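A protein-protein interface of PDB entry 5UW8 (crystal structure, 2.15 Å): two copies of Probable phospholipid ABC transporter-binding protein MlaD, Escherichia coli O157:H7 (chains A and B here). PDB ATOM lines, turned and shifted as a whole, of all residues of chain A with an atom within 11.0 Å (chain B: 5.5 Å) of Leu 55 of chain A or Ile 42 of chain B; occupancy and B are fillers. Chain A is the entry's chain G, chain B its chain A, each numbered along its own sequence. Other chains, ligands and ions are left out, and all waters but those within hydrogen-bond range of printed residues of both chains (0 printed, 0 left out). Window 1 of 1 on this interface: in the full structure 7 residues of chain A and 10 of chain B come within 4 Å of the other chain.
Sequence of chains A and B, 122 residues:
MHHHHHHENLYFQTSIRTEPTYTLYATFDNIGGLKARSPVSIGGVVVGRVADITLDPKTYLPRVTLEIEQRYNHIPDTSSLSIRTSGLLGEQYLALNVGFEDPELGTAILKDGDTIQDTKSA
Of the printed residues of chain B, Asp 29 of chain A touches Gly 43 (3.7 Å).
Of the printed residues of chain B, Ile 53 of chain A touches Val 45.
Leu 55 of chain A touches four residues of chain B.
Val 64 of chain A touches none of the printed residues of chain B.
Printed residues of chain A within 4 Å of Ile 42 of chain B: Leu 55 (3.4 Å) and Tyr 60 (3.7 Å).
Of chain A, only Asp 29 (3.7 Å), Asn 30 (3.6 Å), Ile 31 (3.1 Å) and Pro 62 (3.3 Å) come within 4 Å of Gly 43 of chain B.
Printed residues of chain A within 4 Å of Gly 44 of chain B: Ile 31 (3.7 Å).
Of the printed residues of chain A, Val 45 of chain B touches Ile 53 (3.6 Å), Leu 55 (3.8 Å) and Pro 62 (3.7 Å).
The nearest residue of chain B that does not touch Leu 55 of chain A is Gly 43 of chain B (5.2 Å).
The nearest printed residue of chain A that does not touch Val 47 of chain B is Tyr 60 of chain A (6.4 Å).
The side-chain hydroxyl (OG) of Ser 121 of chain A lies within hydrogen-bond range of the backbone NH (N) of Asn 30 of chain A, at 3.5 Å.
The side-chain amide oxygen of Asn 30 of chain A is in hydrogen-bond range of the backbone NH of Gly 32 of chain A (2.7 Å).
N of Asp 29 of chain A sits at hydrogen-bond distance from OG of Ser 121 of chain A (2.9 Å).
O of Pro 62 of chain A sits at hydrogen-bond distance from N of Phe 28 of chain A (3.1 Å).
The backbone carbonyl oxygen of Val 40 of chain B lies within hydrogen-bond range of the backbone NH of Val 47 of chain B (2.8 Å).
Among the printed residues, pairs that only touch across the chains: Asp 29 of chain A with Gly 43 of chain B (3.7 Å), Asn 30 of chain A with Gly 43 of chain B (3.6 Å), Ile 31 of chain A with Gly 44 of chain B (3.7 Å), Ile 53 of chain A with Val 45 of chain B (3.6 Å), Leu 55 of chain A with Ile 42 of chain B (3.4 Å), Leu 55 of chain A with Val 45 of chain B (3.8 Å), Leu 55 of chain A with Val 47 of chain B (3.9 Å), Tyr 60 of chain A with Ile 42 of chain B (3.7 Å), Tyr 60 of chain A with Tyr 72 of chain B (3.1 Å), Tyr 60 of chain A with Ile 75 of chain B (3.8 Å), Tyr 60 of chain A with Val 98 of chain B (3.96 Å), Pro 62 of chain A with Gly 43 of chain B (3.3 Å) and Pro 62 of chain A with Val 45 of chain B (3.7 Å).
The backbone carbonyl oxygen (O) of Gly 43 of chain B is in hydrogen-bond range of the backbone NH (N) of Ile 31 of chain A (3.1 Å).
The side-chain hydroxyl (OH) of Tyr 72 of chain B lies within hydrogen-bond range of the backbone carbonyl oxygen (O) of Leu 55 of chain A.
No position is printed for both chains.
Of the 15 pairs that touch across the chains among the printed residues, none has its exchanged pair printed and touching as well.
Hydrophobic or aromatic side chains of chain B that line the printed part of chain A: Ile 42, Val 45, Val 47, Tyr 72, Ile 75 and Val 98.
Of the 25 printed residues of chain A, 7 touch a printed residue of chain B.
Along chain A the printed residues that touch a printed residue of chain B span positions 29 to 62.
Among the printed residues, no Asp or Glu carboxylate lies within 4 Å of a Lys or Arg side-chain nitrogen of the other chain.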
ATOM      1  N   TYR A  25     -32.861   0.648 -13.989  1.00  0.00           N
ATOM      2  CA  TYR A  25     -31.668  -0.152 -13.756  1.00  0.00           C
ATOM      3  C   TYR A  25     -31.997  -1.631 -13.891  1.00  0.00           C
ATOM      4  O   TYR A  25     -33.144  -2.039 -13.724  1.00  0.00           O
ATOM      5  CB  TYR A  25     -31.080   0.145 -12.377  1.00  0.00           C
ATOM      6  CG  TYR A  25     -30.753   1.606 -12.165  1.00  0.00           C
ATOM      7  CD1 TYR A  25     -29.596   2.163 -12.697  1.00  0.00           C
ATOM      8  CD2 TYR A  25     -31.600   2.428 -11.432  1.00  0.00           C
ATOM      9  CE1 TYR A  25     -29.292   3.499 -12.505  1.00  0.00           C
ATOM     10  CE2 TYR A  25     -31.305   3.764 -11.236  1.00  0.00           C
ATOM     11  CZ  TYR A  25     -30.150   4.294 -11.774  1.00  0.00           C
ATOM     12  OH  TYR A  25     -29.855   5.624 -11.582  1.00  0.00           O
ATOM     13  N   ALA A  26     -30.985  -2.427 -14.209  1.00  0.00           N
ATOM     14  CA  ALA A  26     -31.145  -3.871 -14.294  1.00  0.00           C
ATOM     15  C   ALA A  26     -29.810  -4.554 -14.046  1.00  0.00           C
ATOM     16  O   ALA A  26     -28.772  -4.107 -14.535  1.00  0.00           O
ATOM     17  CB  ALA A  26     -31.704  -4.269 -15.650  1.00  0.00           C
ATOM     18  N   THR A  27     -29.842  -5.628 -13.265  1.00  0.00           N
ATOM     19  CA  THR A  27     -28.638  -6.389 -12.964  1.00  0.00           C
ATOM     20  C   THR A  27     -28.641  -7.714 -13.718  1.00  0.00           C
ATOM     21  O   THR A  27     -29.643  -8.428 -13.745  1.00  0.00           O
ATOM     22  CB  THR A  27     -28.506  -6.652 -11.453  1.00  0.00           C
ATOM     23  OG1 THR A  27     -28.445  -5.404 -10.754  1.00  0.00           O
ATOM     24  CG2 THR A  27     -27.246  -7.457 -11.151  1.00  0.00           C
ATOM     25  N   PHE A  28     -27.503  -8.021 -14.334  1.00  0.00           N
ATOM     26  CA  PHE A  28     -27.295  -9.285 -15.034  1.00  0.00           C
ATOM     27  C   PHE A  28     -26.117 -10.022 -14.419  1.00  0.00           C
ATOM     28  O   PHE A  28     -25.358  -9.444 -13.647  1.00  0.00           O
ATOM     29  CB  PHE A  28     -27.036  -9.056 -16.523  1.00  0.00           C
ATOM     30  CG  PHE A  28     -28.190  -8.439 -17.256  1.00  0.00           C
ATOM     31  CD1 PHE A  28     -28.417  -7.076 -17.197  1.00  0.00           C
ATOM     32  CD2 PHE A  28     -29.044  -9.224 -18.008  1.00  0.00           C
ATOM     33  CE1 PHE A  28     -29.477  -6.508 -17.876  1.00  0.00           C
ATOM     34  CE2 PHE A  28     -30.106  -8.663 -18.687  1.00  0.00           C
ATOM     35  CZ  PHE A  28     -30.322  -7.303 -18.620  1.00  0.00           C
ATOM     36  N   ASP A  29     -25.988 -11.307 -14.737  1.00  0.00           N
ATOM     37  CA  ASP A  29     -24.802 -12.067 -14.362  1.00  0.00           C
ATOM     38  C   ASP A  29     -23.660 -11.746 -15.322  1.00  0.00           C
ATOM     39  O   ASP A  29     -22.501 -11.656 -14.920  1.00  0.00           O
ATOM     40  CB  ASP A  29     -25.097 -13.568 -14.371  1.00  0.00           C
ATOM     41  CG  ASP A  29     -26.067 -13.980 -13.282  1.00  0.00           C
ATOM     42  OD1 ASP A  29     -26.027 -13.380 -12.187  1.00  0.00           O
ATOM     43  OD2 ASP A  29     -26.872 -14.906 -13.520  1.00  0.00           O
ATOM     44  N   ASN A  30     -24.006 -11.571 -16.593  1.00  0.00           N
ATOM     45  CA  ASN A  30     -23.038 -11.248 -17.634  1.00  0.00           C
ATOM     46  C   ASN A  30     -23.717 -10.451 -18.743  1.00  0.00           C
ATOM     47  O   ASN A  30     -24.734 -10.879 -19.288  1.00  0.00           O
ATOM     48  CB  ASN A  30     -22.403 -12.522 -18.194  1.00  0.00           C
ATOM     49  CG  ASN A  30     -21.188 -12.240 -19.060  1.00  0.00           C
ATOM     50  OD1 ASN A  30     -21.244 -11.434 -19.989  1.00  0.00           O
ATOM     51  ND2 ASN A  30     -20.076 -12.898 -18.750  1.00  0.00           N
ATOM     52  N   ILE A  31     -23.151  -9.294 -19.073  1.00  0.00           N
ATOM     53  CA  ILE A  31     -23.752  -8.409 -20.072  1.00  0.00           C
ATOM     54  C   ILE A  31     -23.274  -8.715 -21.493  1.00  0.00           C
ATOM     55  O   ILE A  31     -23.781  -8.147 -22.454  1.00  0.00           O
ATOM     56  CB  ILE A  31     -23.482  -6.909 -19.741  1.00  0.00           C
ATOM     57  CG1 ILE A  31     -21.988  -6.602 -19.565  1.00  0.00           C
ATOM     58  CG2 ILE A  31     -24.228  -6.510 -18.476  1.00  0.00           C
ATOM     59  CD1 ILE A  31     -21.246  -6.300 -20.842  1.00  0.00           C
ATOM     60  N   GLY A  32     -22.315  -9.624 -21.629  1.00  0.00           N
ATOM     61  CA  GLY A  32     -21.842 -10.044 -22.939  1.00  0.00           C
ATOM     62  C   GLY A  32     -21.305  -8.920 -23.810  1.00  0.00           C
ATOM     63  O   GLY A  32     -20.409  -8.181 -23.407  1.00  0.00           O
ATOM     64  N   GLY A  33     -21.855  -8.799 -25.014  1.00  0.00           N
ATOM     65  CA  GLY A  33     -21.416  -7.791 -25.964  1.00  0.00           C
ATOM     66  C   GLY A  33     -22.176  -6.483 -25.838  1.00  0.00           C
ATOM     67  O   GLY A  33     -22.022  -5.584 -26.665  1.00  0.00           O
ATOM     68  N   LEU A  34     -23.006  -6.381 -24.807  1.00  0.00           N
ATOM     69  CA  LEU A  34     -23.776  -5.168 -24.567  1.00  0.00           C
ATOM     70  C   LEU A  34     -22.830  -4.018 -24.241  1.00  0.00           C
ATOM     71  O   LEU A  34     -21.847  -4.197 -23.523  1.00  0.00           O
ATOM     72  CB  LEU A  34     -24.770  -5.397 -23.427  1.00  0.00           C
ATOM     73  CG  LEU A  34     -26.153  -4.756 -23.465  1.00  0.00           C
ATOM     74  CD1 LEU A  34     -26.922  -5.195 -24.702  1.00  0.00           C
ATOM     75  CD2 LEU A  34     -26.896  -5.158 -22.205  1.00  0.00           C
ATOM     76  N   ASP A  52     -25.248   3.435 -19.721  1.00  0.00           N
ATOM     77  CA  ASP A  52     -24.026   3.130 -18.993  1.00  0.00           C
ATOM     78  C   ASP A  52     -24.054   1.711 -18.428  1.00  0.00           C
ATOM     79  O   ASP A  52     -25.120   1.173 -18.124  1.00  0.00           O
ATOM     80  CB  ASP A  52     -23.828   4.147 -17.866  1.00  0.00           C
ATOM     81  CG  ASP A  52     -22.527   3.945 -17.116  1.00  0.00           C
ATOM     82  OD1 ASP A  52     -21.567   3.410 -17.710  1.00  0.00           O
ATOM     83  OD2 ASP A  52     -22.462   4.328 -15.929  1.00  0.00           O
ATOM     84  N   ILE A  53     -22.873   1.114 -18.291  1.00  0.00           N
ATOM     85  CA  ILE A  53     -22.732  -0.196 -17.660  1.00  0.00           C
ATOM     86  C   ILE A  53     -21.625  -0.143 -16.618  1.00  0.00           C
ATOM     87  O   ILE A  53     -20.490   0.226 -16.921  1.00  0.00           O
ATOM     88  CB  ILE A  53     -22.414  -1.307 -18.679  1.00  0.00           C
ATOM     89  CG1 ILE A  53     -23.472  -1.335 -19.787  1.00  0.00           C
ATOM     90  CG2 ILE A  53     -22.331  -2.661 -17.973  1.00  0.00           C
ATOM     91  CD1 ILE A  53     -23.171  -2.314 -20.907  1.00  0.00           C
ATOM     92  N   THR A  54     -21.970  -0.509 -15.389  1.00  0.00           N
ATOM     93  CA  THR A  54     -21.034  -0.467 -14.274  1.00  0.00           C
ATOM     94  C   THR A  54     -21.180  -1.704 -13.405  1.00  0.00           C
ATOM     95  O   THR A  54     -22.263  -2.280 -13.308  1.00  0.00           O
ATOM     96  CB  THR A  54     -21.259   0.776 -13.400  1.00  0.00           C
ATOM     97  OG1 THR A  54     -22.590   0.752 -12.869  1.00  0.00           O
ATOM     98  CG2 THR A  54     -21.057   2.045 -14.211  1.00  0.00           C
ATOM     99  N   LEU A  55     -20.081  -2.115 -12.782  1.00  0.00           N
ATOM    100  CA  LEU A  55     -20.127  -3.198 -11.813  1.00  0.00           C
ATOM    101  C   LEU A  55     -20.514  -2.666 -10.445  1.00  0.00           C
ATOM    102  O   LEU A  55     -19.939  -1.698  -9.947  1.00  0.00           O
ATOM    103  CB  LEU A  55     -18.783  -3.919 -11.719  1.00  0.00           C
ATOM    104  CG  LEU A  55     -18.871  -5.384 -11.282  1.00  0.00           C
ATOM    105  CD1 LEU A  55     -19.511  -6.251 -12.358  1.00  0.00           C
ATOM    106  CD2 LEU A  55     -17.497  -5.912 -10.904  1.00  0.00           C
ATOM    107  N   ASP A  56     -21.508  -3.305  -9.851  1.00  0.00           N
ATOM    108  CA  ASP A  56     -21.940  -2.986  -8.505  1.00  0.00           C
ATOM    109  C   ASP A  56     -20.847  -3.303  -7.477  1.00  0.00           C
ATOM    110  O   ASP A  56     -20.404  -4.446  -7.390  1.00  0.00           O
ATOM    111  CB  ASP A  56     -23.216  -3.762  -8.203  1.00  0.00           C
ATOM    112  CG  ASP A  56     -23.722  -3.528  -6.801  1.00  0.00           C
ATOM    113  OD1 ASP A  56     -24.239  -2.424  -6.514  1.00  0.00           O
ATOM    114  OD2 ASP A  56     -23.646  -4.480  -6.005  1.00  0.00           O
ATOM    115  N   PRO A  57     -20.410  -2.297  -6.694  1.00  0.00           N
ATOM    116  CA  PRO A  57     -19.264  -2.494  -5.793  1.00  0.00           C
ATOM    117  C   PRO A  57     -19.496  -3.506  -4.661  1.00  0.00           C
ATOM    118  O   PRO A  57     -18.524  -4.085  -4.170  1.00  0.00           O
ATOM    119  CB  PRO A  57     -19.030  -1.087  -5.222  1.00  0.00           C
ATOM    120  CG  PRO A  57     -20.353  -0.430  -5.294  1.00  0.00           C
ATOM    121  CD  PRO A  57     -20.983  -0.945  -6.555  1.00  0.00           C
ATOM    122  N   LYS A  58     -20.749  -3.727  -4.268  1.00  0.00           N
ATOM    123  CA  LYS A  58     -21.049  -4.582  -3.119  1.00  0.00           C
ATOM    124  C   LYS A  58     -21.318  -6.025  -3.578  1.00  0.00           C
ATOM    125  O   LYS A  58     -20.968  -6.970  -2.869  1.00  0.00           O
ATOM    126  CB  LYS A  58     -22.243  -4.021  -2.320  1.00  0.00           C
ATOM    127  CG  LYS A  58     -23.532  -3.909  -3.120  1.00  0.00           C
ATOM    128  CD  LYS A  58     -24.613  -3.051  -2.472  1.00  0.00           C
ATOM    129  CE  LYS A  58     -25.897  -3.115  -3.300  1.00  0.00           C
ATOM    130  NZ  LYS A  58     -26.624  -4.419  -3.171  1.00  0.00           N
ATOM    131  N   THR A  59     -21.917  -6.195  -4.761  1.00  0.00           N
ATOM    132  CA  THR A  59     -22.264  -7.532  -5.272  1.00  0.00           C
ATOM    133  C   THR A  59     -21.360  -8.005  -6.410  1.00  0.00           C
ATOM    134  O   THR A  59     -21.347  -9.189  -6.740  1.00  0.00           O
ATOM    135  CB  THR A  59     -23.717  -7.596  -5.805  1.00  0.00           C
ATOM    136  OG1 THR A  59     -23.847  -6.762  -6.963  1.00  0.00           O
ATOM    137  CG2 THR A  59     -24.704  -7.157  -4.752  1.00  0.00           C
ATOM    138  N   TYR A  60     -20.618  -7.077  -7.008  1.00  0.00           N
ATOM    139  CA  TYR A  60     -19.773  -7.365  -8.167  1.00  0.00           C
ATOM    140  C   TYR A  60     -20.579  -7.965  -9.321  1.00  0.00           C
ATOM    141  O   TYR A  60     -20.069  -8.768 -10.102  1.00  0.00           O
ATOM    142  CB  TYR A  60     -18.627  -8.299  -7.763  1.00  0.00           C
ATOM    143  CG  TYR A  60     -17.544  -7.576  -7.006  1.00  0.00           C
ATOM    144  CD1 TYR A  60     -17.740  -7.187  -5.689  1.00  0.00           C
ATOM    145  CD2 TYR A  60     -16.332  -7.272  -7.606  1.00  0.00           C
ATOM    146  CE1 TYR A  60     -16.761  -6.519  -4.990  1.00  0.00           C
ATOM    147  CE2 TYR A  60     -15.343  -6.603  -6.915  1.00  0.00           C
ATOM    148  CZ  TYR A  60     -15.563  -6.229  -5.608  1.00  0.00           C
ATOM    149  OH  TYR A  60     -14.583  -5.561  -4.913  1.00  0.00           O
ATOM    150  N   LEU A  61     -21.844  -7.566  -9.407  1.00  0.00           N
ATOM    151  CA  LEU A  61     -22.707  -7.930 -10.527  1.00  0.00           C
ATOM    152  C   LEU A  61     -22.879  -6.742 -11.479  1.00  0.00           C
ATOM    153  O   LEU A  61     -23.054  -5.612 -11.025  1.00  0.00           O
ATOM    154  CB  LEU A  61     -24.064  -8.410 -10.016  1.00  0.00           C
ATOM    155  CG  LEU A  61     -24.019  -9.736  -9.247  1.00  0.00           C
ATOM    156  CD1 LEU A  61     -25.378 -10.056  -8.644  1.00  0.00           C
ATOM    157  CD2 LEU A  61     -23.536 -10.889 -10.123  1.00  0.00           C
ATOM    158  N   PRO A  62     -22.811  -6.984 -12.800  1.00  0.00           N
ATOM    159  CA  PRO A  62     -23.032  -5.890 -13.755  1.00  0.00           C
ATOM    160  C   PRO A  62     -24.399  -5.218 -13.611  1.00  0.00           C
ATOM    161  O   PRO A  62     -25.419  -5.907 -13.609  1.00  0.00           O
ATOM    162  CB  PRO A  62     -22.931  -6.585 -15.116  1.00  0.00           C
ATOM    163  CG  PRO A  62     -22.086  -7.770 -14.878  1.00  0.00           C
ATOM    164  CD  PRO A  62     -22.367  -8.218 -13.476  1.00  0.00           C
ATOM    165  N   ARG A  63     -24.405  -3.894 -13.486  1.00  0.00           N
ATOM    166  CA  ARG A  63     -25.639  -3.112 -13.490  1.00  0.00           C
ATOM    167  C   ARG A  63     -25.708  -2.247 -14.739  1.00  0.00           C
ATOM    168  O   ARG A  63     -24.807  -1.449 -14.999  1.00  0.00           O
ATOM    169  CB  ARG A  63     -25.745  -2.223 -12.245  1.00  0.00           C
ATOM    170  CG  ARG A  63     -26.831  -1.150 -12.362  1.00  0.00           C
ATOM    171  CD  ARG A  63     -27.074  -0.386 -11.068  1.00  0.00           C
ATOM    172  NE  ARG A  63     -27.617  -1.237 -10.011  1.00  0.00           N
ATOM    173  CZ  ARG A  63     -26.925  -1.721  -8.983  1.00  0.00           C
ATOM    174  NH1 ARG A  63     -25.633  -1.448  -8.837  1.00  0.00           N
ATOM    175  NH2 ARG A  63     -27.534  -2.484  -8.087  1.00  0.00           N
ATOM    176  N   VAL A  64     -26.792  -2.402 -15.493  1.00  0.00           N
ATOM    177  CA  VAL A  64     -27.025  -1.616 -16.697  1.00  0.00           C
ATOM    178  C   VAL A  64     -27.942  -0.441 -16.382  1.00  0.00           C
ATOM    179  O   VAL A  64     -28.963  -0.608 -15.716  1.00  0.00           O
ATOM    180  CB  VAL A  64     -27.656  -2.471 -17.816  1.00  0.00           C
ATOM    181  CG1 VAL A  64     -27.837  -1.650 -19.084  1.00  0.00           C
ATOM    182  CG2 VAL A  64     -26.804  -3.701 -18.091  1.00  0.00           C
ATOM    183  N   THR A  65     -27.572   0.745 -16.861  1.00  0.00           N
ATOM    184  CA  THR A  65     -28.421   1.922 -16.729  1.00  0.00           C
ATOM    185  C   THR A  65     -29.108   2.165 -18.063  1.00  0.00           C
ATOM    186  O   THR A  65     -28.445   2.391 -19.075  1.00  0.00           O
ATOM    187  CB  THR A  65     -27.619   3.170 -16.313  1.00  0.00           C
ATOM    188  OG1 THR A  65     -26.887   2.896 -15.112  1.00  0.00           O
ATOM    189  CG2 THR A  65     -28.547   4.359 -16.081  1.00  0.00           C
ATOM    190  N   SER A 121     -29.552 -13.361 -18.563  1.00  0.00           N
ATOM    191  CA  SER A 121     -28.254 -13.071 -19.169  1.00  0.00           C
ATOM    192  C   SER A 121     -28.046 -13.920 -20.420  1.00  0.00           C
ATOM    193  O   SER A 121     -28.845 -14.809 -20.717  1.00  0.00           O
ATOM    194  CB  SER A 121     -27.118 -13.309 -18.172  1.00  0.00           C
ATOM    195  OG  SER A 121     -27.313 -12.559 -16.985  1.00  0.00           O
ATOM    196  N   VAL B  40      -9.251  -6.429 -18.275  1.00  0.00           N
ATOM    197  CA  VAL B  40      -9.703  -7.383 -17.274  1.00  0.00           C
ATOM    198  C   VAL B  40     -11.151  -7.041 -16.965  1.00  0.00           C
ATOM    199  O   VAL B  40     -11.466  -5.889 -16.661  1.00  0.00           O
ATOM    200  CB  VAL B  40      -8.851  -7.325 -15.986  1.00  0.00           C
ATOM    201  CG1 VAL B  40      -9.352  -8.334 -14.958  1.00  0.00           C
ATOM    202  CG2 VAL B  40      -7.384  -7.566 -16.307  1.00  0.00           C
ATOM    203  N   SER B  41     -12.031  -8.033 -17.047  1.00  0.00           N
ATOM    204  CA  SER B  41     -13.459  -7.784 -16.890  1.00  0.00           C
ATOM    205  C   SER B  41     -14.125  -8.751 -15.923  1.00  0.00           C
ATOM    206  O   SER B  41     -13.701  -9.897 -15.779  1.00  0.00           O
ATOM    207  CB  SER B  41     -14.151  -7.857 -18.252  1.00  0.00           C
ATOM    208  OG  SER B  41     -14.084  -9.170 -18.786  1.00  0.00           O
ATOM    209  N   ILE B  42     -15.175  -8.265 -15.267  1.00  0.00           N
ATOM    210  CA  ILE B  42     -16.042  -9.089 -14.433  1.00  0.00           C
ATOM    211  C   ILE B  42     -17.458  -9.015 -14.983  1.00  0.00           C
ATOM    212  O   ILE B  42     -18.075  -7.951 -14.987  1.00  0.00           O
ATOM    213  CB  ILE B  42     -16.026  -8.641 -12.955  1.00  0.00           C
ATOM    214  CG1 ILE B  42     -14.617  -8.801 -12.376  1.00  0.00           C
ATOM    215  CG2 ILE B  42     -17.027  -9.454 -12.137  1.00  0.00           C
ATOM    216  CD1 ILE B  42     -14.446  -8.251 -10.971  1.00  0.00           C
ATOM    217  N   GLY B  43     -17.966 -10.153 -15.443  1.00  0.00           N
ATOM    218  CA  GLY B  43     -19.286 -10.214 -16.037  1.00  0.00           C
ATOM    219  C   GLY B  43     -19.394  -9.327 -17.262  1.00  0.00           C
ATOM    220  O   GLY B  43     -20.453  -8.774 -17.543  1.00  0.00           O
ATOM    221  N   GLY B  44     -18.285  -9.187 -17.985  1.00  0.00           N
ATOM    222  CA  GLY B  44     -18.254  -8.406 -19.209  1.00  0.00           C
ATOM    223  C   GLY B  44     -17.930  -6.942 -18.977  1.00  0.00           C
ATOM    224  O   GLY B  44     -17.647  -6.209 -19.925  1.00  0.00           O
ATOM    225  N   VAL B  45     -17.968  -6.515 -17.719  1.00  0.00           N
ATOM    226  CA  VAL B  45     -17.656  -5.133 -17.371  1.00  0.00           C
ATOM    227  C   VAL B  45     -16.170  -4.991 -17.079  1.00  0.00           C
ATOM    228  O   VAL B  45     -15.640  -5.665 -16.198  1.00  0.00           O
ATOM    229  CB  VAL B  45     -18.458  -4.663 -16.140  1.00  0.00           C
ATOM    230  CG1 VAL B  45     -18.159  -3.201 -15.829  1.00  0.00           C
ATOM    231  CG2 VAL B  45     -19.948  -4.866 -16.369  1.00  0.00           C
ATOM    232  N   VAL B  46     -15.503  -4.103 -17.809  1.00  0.00           N
ATOM    233  CA  VAL B  46     -14.071  -3.895 -17.631  1.00  0.00           C
ATOM    234  C   VAL B  46     -13.789  -3.200 -16.304  1.00  0.00           C
ATOM    235  O   VAL B  46     -14.310  -2.118 -16.038  1.00  0.00           O
ATOM    236  CB  VAL B  46     -13.473  -3.069 -18.789  1.00  0.00           C
ATOM    237  CG1 VAL B  46     -11.973  -2.866 -18.595  1.00  0.00           C
ATOM    238  CG2 VAL B  46     -13.751  -3.750 -20.122  1.00  0.00           C
ATOM    239  N   VAL B  47     -12.956  -3.833 -15.483  1.00  0.00           N
ATOM    240  CA  VAL B  47     -12.613  -3.314 -14.162  1.00  0.00           C
ATOM    241  C   VAL B  47     -11.110  -3.095 -14.015  1.00  0.00           C
ATOM    242  O   VAL B  47     -10.651  -2.552 -13.010  1.00  0.00           O
ATOM    243  CB  VAL B  47     -13.093  -4.262 -13.047  1.00  0.00           C
ATOM    244  CG1 VAL B  47     -14.612  -4.341 -13.040  1.00  0.00           C
ATOM    245  CG2 VAL B  47     -12.478  -5.648 -13.214  1.00  0.00           C
ATOM    246  N   TYR B  72     -12.995  -1.640  -6.617  1.00  0.00           N
ATOM    247  CA  TYR B  72     -13.255  -3.075  -6.598  1.00  0.00           C
ATOM    248  C   TYR B  72     -12.147  -3.795  -5.831  1.00  0.00           C
ATOM    249  O   TYR B  72     -11.375  -4.560  -6.410  1.00  0.00           O
ATOM    250  CB  TYR B  72     -13.382  -3.614  -8.024  1.00  0.00           C
ATOM    251  CG  TYR B  72     -14.402  -2.856  -8.842  1.00  0.00           C
ATOM    252  CD1 TYR B  72     -15.748  -2.898  -8.509  1.00  0.00           C
ATOM    253  CD2 TYR B  72     -14.021  -2.095  -9.940  1.00  0.00           C
ATOM    254  CE1 TYR B  72     -16.689  -2.201  -9.242  1.00  0.00           C
ATOM    255  CE2 TYR B  72     -14.955  -1.395 -10.682  1.00  0.00           C
ATOM    256  CZ  TYR B  72     -16.288  -1.453 -10.330  1.00  0.00           C
ATOM    257  OH  TYR B  72     -17.222  -0.762 -11.066  1.00  0.00           O
ATOM    258  N   ILE B  75     -12.313  -8.386  -3.804  1.00  0.00           N
ATOM    259  CA  ILE B  75     -12.250  -9.596  -4.616  1.00  0.00           C
ATOM    260  C   ILE B  75     -11.699 -10.756  -3.785  1.00  0.00           C
ATOM    261  O   ILE B  75     -10.580 -10.673  -3.279  1.00  0.00           O
ATOM    262  CB  ILE B  75     -11.381  -9.389  -5.868  1.00  0.00           C
ATOM    263  CG1 ILE B  75     -11.964  -8.254  -6.714  1.00  0.00           C
ATOM    264  CG2 ILE B  75     -11.308 -10.673  -6.691  1.00  0.00           C
ATOM    265  CD1 ILE B  75     -11.124  -7.862  -7.910  1.00  0.00           C
ATOM    266  N   LEU B  96     -12.288 -12.263 -15.049  1.00  0.00           N
ATOM    267  CA  LEU B  96     -12.141 -12.534 -13.627  1.00  0.00           C
ATOM    268  C   LEU B  96     -13.458 -13.052 -13.074  1.00  0.00           C
ATOM    269  O   LEU B  96     -14.463 -12.342 -13.068  1.00  0.00           O
ATOM    270  CB  LEU B  96     -11.698 -11.279 -12.870  1.00  0.00           C
ATOM    271  CG  LEU B  96     -11.139 -11.504 -11.458  1.00  0.00           C
ATOM    272  CD1 LEU B  96     -10.293 -10.319 -11.030  1.00  0.00           C
ATOM    273  CD2 LEU B  96     -12.245 -11.748 -10.433  1.00  0.00           C
ATOM    274  N   VAL B  98     -15.449 -13.935  -9.956  1.00  0.00           N
ATOM    275  CA  VAL B  98     -15.470 -13.658  -8.527  1.00  0.00           C
ATOM    276  C   VAL B  98     -15.668 -14.971  -7.793  1.00  0.00           C
ATOM    277  O   VAL B  98     -16.648 -15.680  -8.019  1.00  0.00           O
ATOM    278  CB  VAL B  98     -16.580 -12.655  -8.156  1.00  0.00           C
ATOM    279  CG1 VAL B  98     -16.590 -12.386  -6.655  1.00  0.00           C
ATOM    280  CG2 VAL B  98     -16.392 -11.356  -8.927  1.00  0.00           C
